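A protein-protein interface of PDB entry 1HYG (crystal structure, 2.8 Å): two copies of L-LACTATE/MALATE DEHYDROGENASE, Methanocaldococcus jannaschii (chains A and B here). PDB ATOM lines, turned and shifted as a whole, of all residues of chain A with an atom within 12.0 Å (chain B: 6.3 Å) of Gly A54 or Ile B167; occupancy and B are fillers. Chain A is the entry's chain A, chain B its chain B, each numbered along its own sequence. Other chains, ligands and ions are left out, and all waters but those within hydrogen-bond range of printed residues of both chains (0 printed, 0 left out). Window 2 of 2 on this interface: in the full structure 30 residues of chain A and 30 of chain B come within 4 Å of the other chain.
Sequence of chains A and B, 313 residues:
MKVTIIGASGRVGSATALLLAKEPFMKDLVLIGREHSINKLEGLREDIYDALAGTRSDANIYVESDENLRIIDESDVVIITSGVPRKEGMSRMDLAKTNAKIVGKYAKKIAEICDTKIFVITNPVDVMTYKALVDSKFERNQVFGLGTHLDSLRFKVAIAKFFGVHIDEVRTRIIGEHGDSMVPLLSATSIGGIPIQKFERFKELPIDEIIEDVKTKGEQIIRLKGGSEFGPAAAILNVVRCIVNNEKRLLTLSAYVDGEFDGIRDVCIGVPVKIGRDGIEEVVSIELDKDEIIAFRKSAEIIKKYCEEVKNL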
ATOM      1  N   LEU A  18       8.107  17.379  -5.781  1.00  0.00           N
ATOM      2  CA  LEU A  18       7.808  18.726  -5.307  1.00  0.00           C
ATOM      3  C   LEU A  18       6.425  19.118  -5.802  1.00  0.00           C
ATOM      4  O   LEU A  18       5.521  19.374  -5.011  1.00  0.00           O
ATOM      5  CB  LEU A  18       8.864  19.721  -5.825  1.00  0.00           C
ATOM      6  CG  LEU A  18       8.912  21.158  -5.263  1.00  0.00           C
ATOM      7  CD1 LEU A  18       8.189  22.127  -6.195  1.00  0.00           C
ATOM      8  CD2 LEU A  18       8.297  21.187  -3.851  1.00  0.00           C
ATOM      9  N   ALA A  21       3.501  16.988  -4.397  1.00  0.00           N
ATOM     10  CA  ALA A  21       3.158  17.210  -2.986  1.00  0.00           C
ATOM     11  C   ALA A  21       2.237  18.421  -2.816  1.00  0.00           C
ATOM     12  O   ALA A  21       1.473  18.498  -1.852  1.00  0.00           O
ATOM     13  CB  ALA A  21       4.418  17.403  -2.150  1.00  0.00           C
ATOM     14  N   LYS A  22       2.310  19.367  -3.748  1.00  0.00           N
ATOM     15  CA  LYS A  22       1.469  20.553  -3.671  1.00  0.00           C
ATOM     16  C   LYS A  22       0.039  20.274  -4.117  1.00  0.00           C
ATOM     17  O   LYS A  22      -0.874  21.002  -3.744  1.00  0.00           O
ATOM     18  CB  LYS A  22       2.056  21.689  -4.511  1.00  0.00           C
ATOM     19  CG  LYS A  22       3.362  22.251  -3.980  1.00  0.00           C
ATOM     20  CD  LYS A  22       3.878  23.404  -4.845  1.00  0.00           C
ATOM     21  CE  LYS A  22       5.248  23.928  -4.360  1.00  0.00           C
ATOM     22  NZ  LYS A  22       5.211  24.594  -3.008  1.00  0.00           N
ATOM     23  N   GLU A  46      12.243  16.591   3.648  1.00  0.00           N
ATOM     24  CA  GLU A  46      12.301  17.755   4.515  1.00  0.00           C
ATOM     25  C   GLU A  46      12.253  19.026   3.682  1.00  0.00           C
ATOM     26  O   GLU A  46      11.587  19.992   4.048  1.00  0.00           O
ATOM     27  CB  GLU A  46      13.577  17.736   5.365  1.00  0.00           C
ATOM     28  CG  GLU A  46      13.621  16.681   6.466  1.00  0.00           C
ATOM     29  CD  GLU A  46      12.466  16.804   7.451  1.00  0.00           C
ATOM     30  OE1 GLU A  46      11.970  17.940   7.645  1.00  0.00           O
ATOM     31  OE2 GLU A  46      12.063  15.768   8.037  1.00  0.00           O
ATOM     32  N   ASP A  47      12.957  19.032   2.559  1.00  0.00           N
ATOM     33  CA  ASP A  47      12.984  20.217   1.693  1.00  0.00           C
ATOM     34  C   ASP A  47      11.599  20.549   1.147  1.00  0.00           C
ATOM     35  O   ASP A  47      11.144  21.683   1.236  1.00  0.00           O
ATOM     36  CB  ASP A  47      13.950  20.005   0.524  1.00  0.00           C
ATOM     37  CG  ASP A  47      14.372  21.308  -0.126  1.00  0.00           C
ATOM     38  OD1 ASP A  47      14.936  21.255  -1.233  1.00  0.00           O
ATOM     39  OD2 ASP A  47      14.153  22.382   0.475  1.00  0.00           O
ATOM     40  N   ILE A  48      10.937  19.556   0.561  1.00  0.00           N
ATOM     41  CA  ILE A  48       9.594  19.747   0.029  1.00  0.00           C
ATOM     42  C   ILE A  48       8.698  20.340   1.122  1.00  0.00           C
ATOM     43  O   ILE A  48       8.024  21.351   0.895  1.00  0.00           O
ATOM     44  CB  ILE A  48       8.997  18.399  -0.474  1.00  0.00           C
ATOM     45  CG1 ILE A  48       9.696  17.970  -1.766  1.00  0.00           C
ATOM     46  CG2 ILE A  48       7.497  18.523  -0.700  1.00  0.00           C
ATOM     47  CD1 ILE A  48       9.301  16.574  -2.244  1.00  0.00           C
ATOM     48  N   TYR A  49       8.710  19.727   2.309  1.00  0.00           N
ATOM     49  CA  TYR A  49       7.890  20.201   3.432  1.00  0.00           C
ATOM     50  C   TYR A  49       8.064  21.692   3.682  1.00  0.00           C
ATOM     51  O   TYR A  49       7.117  22.369   4.067  1.00  0.00           O
ATOM     52  CB  TYR A  49       8.202  19.413   4.717  1.00  0.00           C
ATOM     53  CG  TYR A  49       7.434  18.109   4.837  1.00  0.00           C
ATOM     54  CD1 TYR A  49       6.038  18.100   4.878  1.00  0.00           C
ATOM     55  CD2 TYR A  49       8.095  16.879   4.882  1.00  0.00           C
ATOM     56  CE1 TYR A  49       5.322  16.898   4.956  1.00  0.00           C
ATOM     57  CE2 TYR A  49       7.383  15.672   4.962  1.00  0.00           C
ATOM     58  CZ  TYR A  49       6.002  15.691   4.997  1.00  0.00           C
ATOM     59  OH  TYR A  49       5.302  14.508   5.080  1.00  0.00           O
ATOM     60  N   ASP A  50       9.273  22.199   3.461  1.00  0.00           N
ATOM     61  CA  ASP A  50       9.548  23.617   3.647  1.00  0.00           C
ATOM     62  C   ASP A  50       8.835  24.427   2.579  1.00  0.00           C
ATOM     63  O   ASP A  50       8.279  25.486   2.859  1.00  0.00           O
ATOM     64  CB  ASP A  50      11.050  23.914   3.558  1.00  0.00           C
ATOM     65  CG  ASP A  50      11.814  23.527   4.819  1.00  0.00           C
ATOM     66  OD1 ASP A  50      11.195  23.353   5.896  1.00  0.00           O
ATOM     67  OD2 ASP A  50      13.053  23.418   4.725  1.00  0.00           O
ATOM     68  N   ALA A  51       8.865  23.931   1.349  1.00  0.00           N
ATOM     69  CA  ALA A  51       8.215  24.618   0.247  1.00  0.00           C
ATOM     70  C   ALA A  51       6.700  24.645   0.456  1.00  0.00           C
ATOM     71  O   ALA A  51       6.002  25.478  -0.120  1.00  0.00           O
ATOM     72  CB  ALA A  51       8.560  23.936  -1.067  1.00  0.00           C
ATOM     73  N   LEU A  52       6.199  23.737   1.288  1.00  0.00           N
ATOM     74  CA  LEU A  52       4.770  23.663   1.575  1.00  0.00           C
ATOM     75  C   LEU A  52       4.389  24.462   2.816  1.00  0.00           C
ATOM     76  O   LEU A  52       3.217  24.679   3.088  1.00  0.00           O
ATOM     77  CB  LEU A  52       4.363  22.210   1.780  1.00  0.00           C
ATOM     78  CG  LEU A  52       3.553  21.487   0.700  1.00  0.00           C
ATOM     79  CD1 LEU A  52       3.959  21.931  -0.693  1.00  0.00           C
ATOM     80  CD2 LEU A  52       3.762  19.986   0.863  1.00  0.00           C
ATOM     81  N   ALA A  53       5.385  24.905   3.565  1.00  0.00           N
ATOM     82  CA  ALA A  53       5.136  25.641   4.787  1.00  0.00           C
ATOM     83  C   ALA A  53       4.251  26.870   4.598  1.00  0.00           C
ATOM     84  O   ALA A  53       4.686  27.860   4.019  1.00  0.00           O
ATOM     85  CB  ALA A  53       6.462  26.040   5.413  1.00  0.00           C
ATOM     86  N   GLY A  54       3.018  26.808   5.100  1.00  0.00           N
ATOM     87  CA  GLY A  54       2.105  27.941   4.979  1.00  0.00           C
ATOM     88  C   GLY A  54       0.861  27.652   4.148  1.00  0.00           C
ATOM     89  O   GLY A  54      -0.171  28.324   4.266  1.00  0.00           O
ATOM     90  N   THR A  55       0.969  26.643   3.295  1.00  0.00           N
ATOM     91  CA  THR A  55      -0.126  26.238   2.437  1.00  0.00           C
ATOM     92  C   THR A  55      -0.713  24.938   2.963  1.00  0.00           C
ATOM     93  O   THR A  55       0.002  24.121   3.543  1.00  0.00           O
ATOM     94  CB  THR A  55       0.369  26.021   1.011  1.00  0.00           C
ATOM     95  OG1 THR A  55       1.532  25.185   1.040  1.00  0.00           O
ATOM     96  CG2 THR A  55       0.722  27.349   0.361  1.00  0.00           C
ATOM     97  N   ARG A  56      -2.015  24.748   2.765  1.00  0.00           N
ATOM     98  CA  ARG A  56      -2.686  23.536   3.224  1.00  0.00           C
ATOM     99  C   ARG A  56      -2.124  22.356   2.436  1.00  0.00           C
ATOM    100  O   ARG A  56      -1.833  22.471   1.240  1.00  0.00           O
ATOM    101  CB  ARG A  56      -4.202  23.651   3.001  1.00  0.00           C
ATOM    102  CG  ARG A  56      -5.088  22.875   3.997  1.00  0.00           C
ATOM    103  CD  ARG A  56      -4.824  21.368   3.974  1.00  0.00           C
ATOM    104  NE  ARG A  56      -5.992  20.559   3.592  1.00  0.00           N
ATOM    105  CZ  ARG A  56      -7.141  20.504   4.266  1.00  0.00           C
ATOM    106  NH1 ARG A  56      -8.129  19.732   3.833  1.00  0.00           N
ATOM    107  NH2 ARG A  56      -7.308  21.223   5.369  1.00  0.00           N
ATOM    108  N   SER A  57      -1.952  21.227   3.115  1.00  0.00           N
ATOM    109  CA  SER A  57      -1.443  20.022   2.474  1.00  0.00           C
ATOM    110  C   SER A  57      -1.517  18.851   3.446  1.00  0.00           C
ATOM    111  O   SER A  57      -1.165  18.979   4.619  1.00  0.00           O
ATOM    112  CB  SER A  57      -0.001  20.225   2.033  1.00  0.00           C
ATOM    113  OG  SER A  57       0.812  20.483   3.161  1.00  0.00           O
ATOM    114  N   ASP A  58      -1.990  17.714   2.954  1.00  0.00           N
ATOM    115  CA  ASP A  58      -2.099  16.522   3.779  1.00  0.00           C
ATOM    116  C   ASP A  58      -1.187  15.475   3.161  1.00  0.00           C
ATOM    117  O   ASP A  58      -1.314  14.276   3.431  1.00  0.00           O
ATOM    118  CB  ASP A  58      -3.542  16.012   3.804  1.00  0.00           C
ATOM    119  CG  ASP A  58      -4.524  17.063   4.292  1.00  0.00           C
ATOM    120  OD1 ASP A  58      -4.390  17.518   5.450  1.00  0.00           O
ATOM    121  OD2 ASP A  58      -5.430  17.431   3.513  1.00  0.00           O
ATOM    122  N   ALA A  59      -0.260  15.947   2.332  1.00  0.00           N
ATOM    123  CA  ALA A  59       0.688  15.074   1.649  1.00  0.00           C
ATOM    124  C   ALA A  59       1.649  14.357   2.594  1.00  0.00           C
ATOM    125  O   ALA A  59       2.542  14.970   3.184  1.00  0.00           O
ATOM    126  CB  ALA A  59       1.477  15.874   0.615  1.00  0.00           C
ATOM    127  N   LEU B 153       7.588  30.371   9.260  1.00  0.00           N
ATOM    128  CA  LEU B 153       6.556  29.514   8.683  1.00  0.00           C
ATOM    129  C   LEU B 153       6.680  28.116   9.279  1.00  0.00           C
ATOM    130  O   LEU B 153       5.676  27.483   9.613  1.00  0.00           O
ATOM    131  CB  LEU B 153       6.687  29.441   7.157  1.00  0.00           C
ATOM    132  CG  LEU B 153       6.441  30.727   6.359  1.00  0.00           C
ATOM    133  CD1 LEU B 153       6.815  30.490   4.900  1.00  0.00           C
ATOM    134  CD2 LEU B 153       4.989  31.156   6.488  1.00  0.00           C
ATOM    135  N   LYS B 156       5.116  28.009  12.551  1.00  0.00           N
ATOM    136  CA  LYS B 156       3.681  28.126  12.323  1.00  0.00           C
ATOM    137  C   LYS B 156       3.060  26.759  12.066  1.00  0.00           C
ATOM    138  O   LYS B 156       2.048  26.404  12.664  1.00  0.00           O
ATOM    139  CB  LYS B 156       3.441  29.027  11.115  1.00  0.00           C
ATOM    140  CG  LYS B 156       2.043  28.980  10.552  1.00  0.00           C
ATOM    141  CD  LYS B 156       1.901  29.980   9.415  1.00  0.00           C
ATOM    142  CE  LYS B 156       0.484  30.004   8.880  1.00  0.00           C
ATOM    143  NZ  LYS B 156       0.164  31.312   8.245  1.00  0.00           N
ATOM    144  N   VAL B 157       3.671  25.994  11.168  1.00  0.00           N
ATOM    145  CA  VAL B 157       3.176  24.667  10.837  1.00  0.00           C
ATOM    146  C   VAL B 157       3.164  23.796  12.069  1.00  0.00           C
ATOM    147  O   VAL B 157       2.143  23.225  12.419  1.00  0.00           O
ATOM    148  CB  VAL B 157       4.051  23.963   9.796  1.00  0.00           C
ATOM    149  CG1 VAL B 157       3.469  22.608   9.490  1.00  0.00           C
ATOM    150  CG2 VAL B 157       4.135  24.785   8.527  1.00  0.00           C
ATOM    151  N   ALA B 160       0.242  24.883  14.455  1.00  0.00           N
ATOM    152  CA  ALA B 160      -1.065  24.588  13.881  1.00  0.00           C
ATOM    153  C   ALA B 160      -1.323  23.092  13.928  1.00  0.00           C
ATOM    154  O   ALA B 160      -2.451  22.650  14.136  1.00  0.00           O
ATOM    155  CB  ALA B 160      -1.130  25.075  12.431  1.00  0.00           C
ATOM    156  N   VAL B 165      -5.465  22.747  14.017  1.00  0.00           N
ATOM    157  CA  VAL B 165      -6.242  23.834  13.436  1.00  0.00           C
ATOM    158  C   VAL B 165      -5.674  24.104  12.056  1.00  0.00           C
ATOM    159  O   VAL B 165      -4.503  23.805  11.787  1.00  0.00           O
ATOM    160  CB  VAL B 165      -6.151  25.153  14.273  1.00  0.00           C
ATOM    161  CG1 VAL B 165      -6.604  24.901  15.694  1.00  0.00           C
ATOM    162  CG2 VAL B 165      -4.727  25.710  14.255  1.00  0.00           C
ATOM    163  N   HIS B 166      -6.510  24.661  11.186  1.00  0.00           N
ATOM    164  CA  HIS B 166      -6.093  24.979   9.828  1.00  0.00           C
ATOM    165  C   HIS B 166      -4.840  25.861   9.856  1.00  0.00           C
ATOM    166  O   HIS B 166      -4.704  26.771  10.682  1.00  0.00           O
ATOM    167  CB  HIS B 166      -7.231  25.682   9.080  1.00  0.00           C
ATOM    168  CG  HIS B 166      -7.004  25.803   7.606  1.00  0.00           C
ATOM    169  ND1 HIS B 166      -6.169  26.752   7.050  1.00  0.00           N
ATOM    170  CD2 HIS B 166      -7.469  25.059   6.571  1.00  0.00           C
ATOM    171  CE1 HIS B 166      -6.128  26.587   5.739  1.00  0.00           C
ATOM    172  NE2 HIS B 166      -6.908  25.566   5.422  1.00  0.00           N
ATOM    173  N   ILE B 167      -3.918  25.570   8.949  1.00  0.00           N
ATOM    174  CA  ILE B 167      -2.672  26.318   8.864  1.00  0.00           C
ATOM    175  C   ILE B 167      -2.899  27.832   8.930  1.00  0.00           C
ATOM    176  O   ILE B 167      -2.147  28.556   9.589  1.00  0.00           O
ATOM    177  CB  ILE B 167      -1.920  25.965   7.558  1.00  0.00           C
ATOM    178  CG1 ILE B 167      -0.611  26.743   7.478  1.00  0.00           C
ATOM    179  CG2 ILE B 167      -2.797  26.260   6.361  1.00  0.00           C
ATOM    180  CD1 ILE B 167       0.367  26.404   8.592  1.00  0.00           C
ATOM    181  N   ASP B 168      -3.944  28.309   8.262  1.00  0.00           N
ATOM    182  CA  ASP B 168      -4.236  29.739   8.244  1.00  0.00           C
ATOM    183  C   ASP B 168      -4.608  30.357   9.576  1.00  0.00           C
ATOM    184  O   ASP B 168      -4.432  31.554   9.760  1.00  0.00           O
ATOM    185  CB  ASP B 168      -5.342  30.044   7.237  1.00  0.00           C
ATOM    186  CG  ASP B 168      -4.862  29.965   5.822  1.00  0.00           C
ATOM    187  OD1 ASP B 168      -3.622  29.904   5.632  1.00  0.00           O
ATOM    188  OD2 ASP B 168      -5.712  29.979   4.903  1.00  0.00           O
ATOM    189  N   GLU B 169      -5.115  29.550  10.500  1.00  0.00           N
ATOM    190  CA  GLU B 169      -5.541  30.056  11.798  1.00  0.00           C
ATOM    191  C   GLU B 169      -4.394  30.413  12.724  1.00  0.00           C
ATOM    192  O   GLU B 169      -4.619  30.901  13.826  1.00  0.00           O
ATOM    193  CB  GLU B 169      -6.447  29.030  12.489  1.00  0.00           C
ATOM    194  CG  GLU B 169      -7.845  28.876  11.894  1.00  0.00           C
ATOM    195  CD  GLU B 169      -8.647  30.144  11.985  1.00  0.00           C
ATOM    196  OE1 GLU B 169      -8.334  30.951  12.867  1.00  0.00           O
ATOM    197  OE2 GLU B 169      -9.590  30.336  11.192  1.00  0.00           O
ATOM    198  N   VAL B 170      -3.163  30.168  12.284  1.00  0.00           N
ATOM    199  CA  VAL B 170      -1.992  30.480  13.103  1.00  0.00           C
ATOM    200  C   VAL B 170      -1.097  31.543  12.474  1.00  0.00           C
ATOM    201  O   VAL B 170      -0.924  31.615  11.249  1.00  0.00           O
ATOM    202  CB  VAL B 170      -1.109  29.219  13.382  1.00  0.00           C
ATOM    203  CG1 VAL B 170       0.169  29.625  14.108  1.00  0.00           C
ATOM    204  CG2 VAL B 170      -1.866  28.214  14.236  1.00  0.00           C
ATOM    205  N   ARG B 171      -0.543  32.377  13.336  1.00  0.00           N
ATOM    206  CA  ARG B 171       0.359  33.420  12.918  1.00  0.00           C
ATOM    207  C   ARG B 171       1.316  33.576  14.081  1.00  0.00           C
ATOM    208  O   ARG B 171       0.919  33.937  15.189  1.00  0.00           O
ATOM    209  CB  ARG B 171      -0.381  34.727  12.662  1.00  0.00           C
ATOM    210  CG  ARG B 171       0.516  35.827  12.092  1.00  0.00           C
ATOM    211  CD  ARG B 171       1.159  35.412  10.770  1.00  0.00           C
ATOM    212  NE  ARG B 171       1.887  36.500  10.119  1.00  0.00           N
ATOM    213  CZ  ARG B 171       3.188  36.745  10.256  1.00  0.00           C
ATOM    214  NH1 ARG B 171       3.734  37.763   9.608  1.00  0.00           N
ATOM    215  NH2 ARG B 171       3.950  35.979  11.023  1.00  0.00           N
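No position is printed for both chains.
Of the 5 pairs that touch across the chains among the printed residues, none has its exchanged pair printed and touching as well.
Hydrophobic or aromatic side chains of chain A that line the printed part of chain B: Ala A53.
Of the 11 printed residues of chain B, 4 touch a printed residue of chain A.
N of Asp B168 sits at hydrogen-bond distance from ND1 of His B166 (3.0 Å).
The guanidinium group (NE) of Arg A56 lies within salt-bridge range of the side-chain carboxylate (OD2) of Asp A58, 3.2 Å away.
Among the printed residues, merely in contact across the chains: Ala A53 with Leu B153, Ala A53 with Val B157, Gly A54 with Ile B167, Arg A56 with His B166 and Arg A56 with Ile B167.
Gly A54 touches just one residue of chain B: Ile B167 (3.6 Å).
Ile B167 touches just these residues of chain A: Gly A54 and Arg A56.
No residue of chain A comes within 4 Å of Lys B156.
Val B157 touches just one residue of chain A: Ala A53 (3.97 Å).
No residue of chain A comes within 4 Å of Ala B160.
Val B165 touches none of the printed residues of chain A.
His B166 touches one residue of chain A.
No residue of chain A comes within 4 Å of Asp B168.
No residue of chain A comes within 4 Å of Val B170.
Printed residues of chain B within 4 Å of Ala A53: Leu B153 (3.5 Å) and Val B157 (3.97 Å).
Printed residues of chain B within 4 Å of Arg A56: His B166 and Ile B167.
Glu A46 touches none of the printed residues of chain B.
Thr A55 touches none of the printed residues of chain B.
The nearest residue of chain B that does not touch Gly A54 is Asp B168 (4.03 Å).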
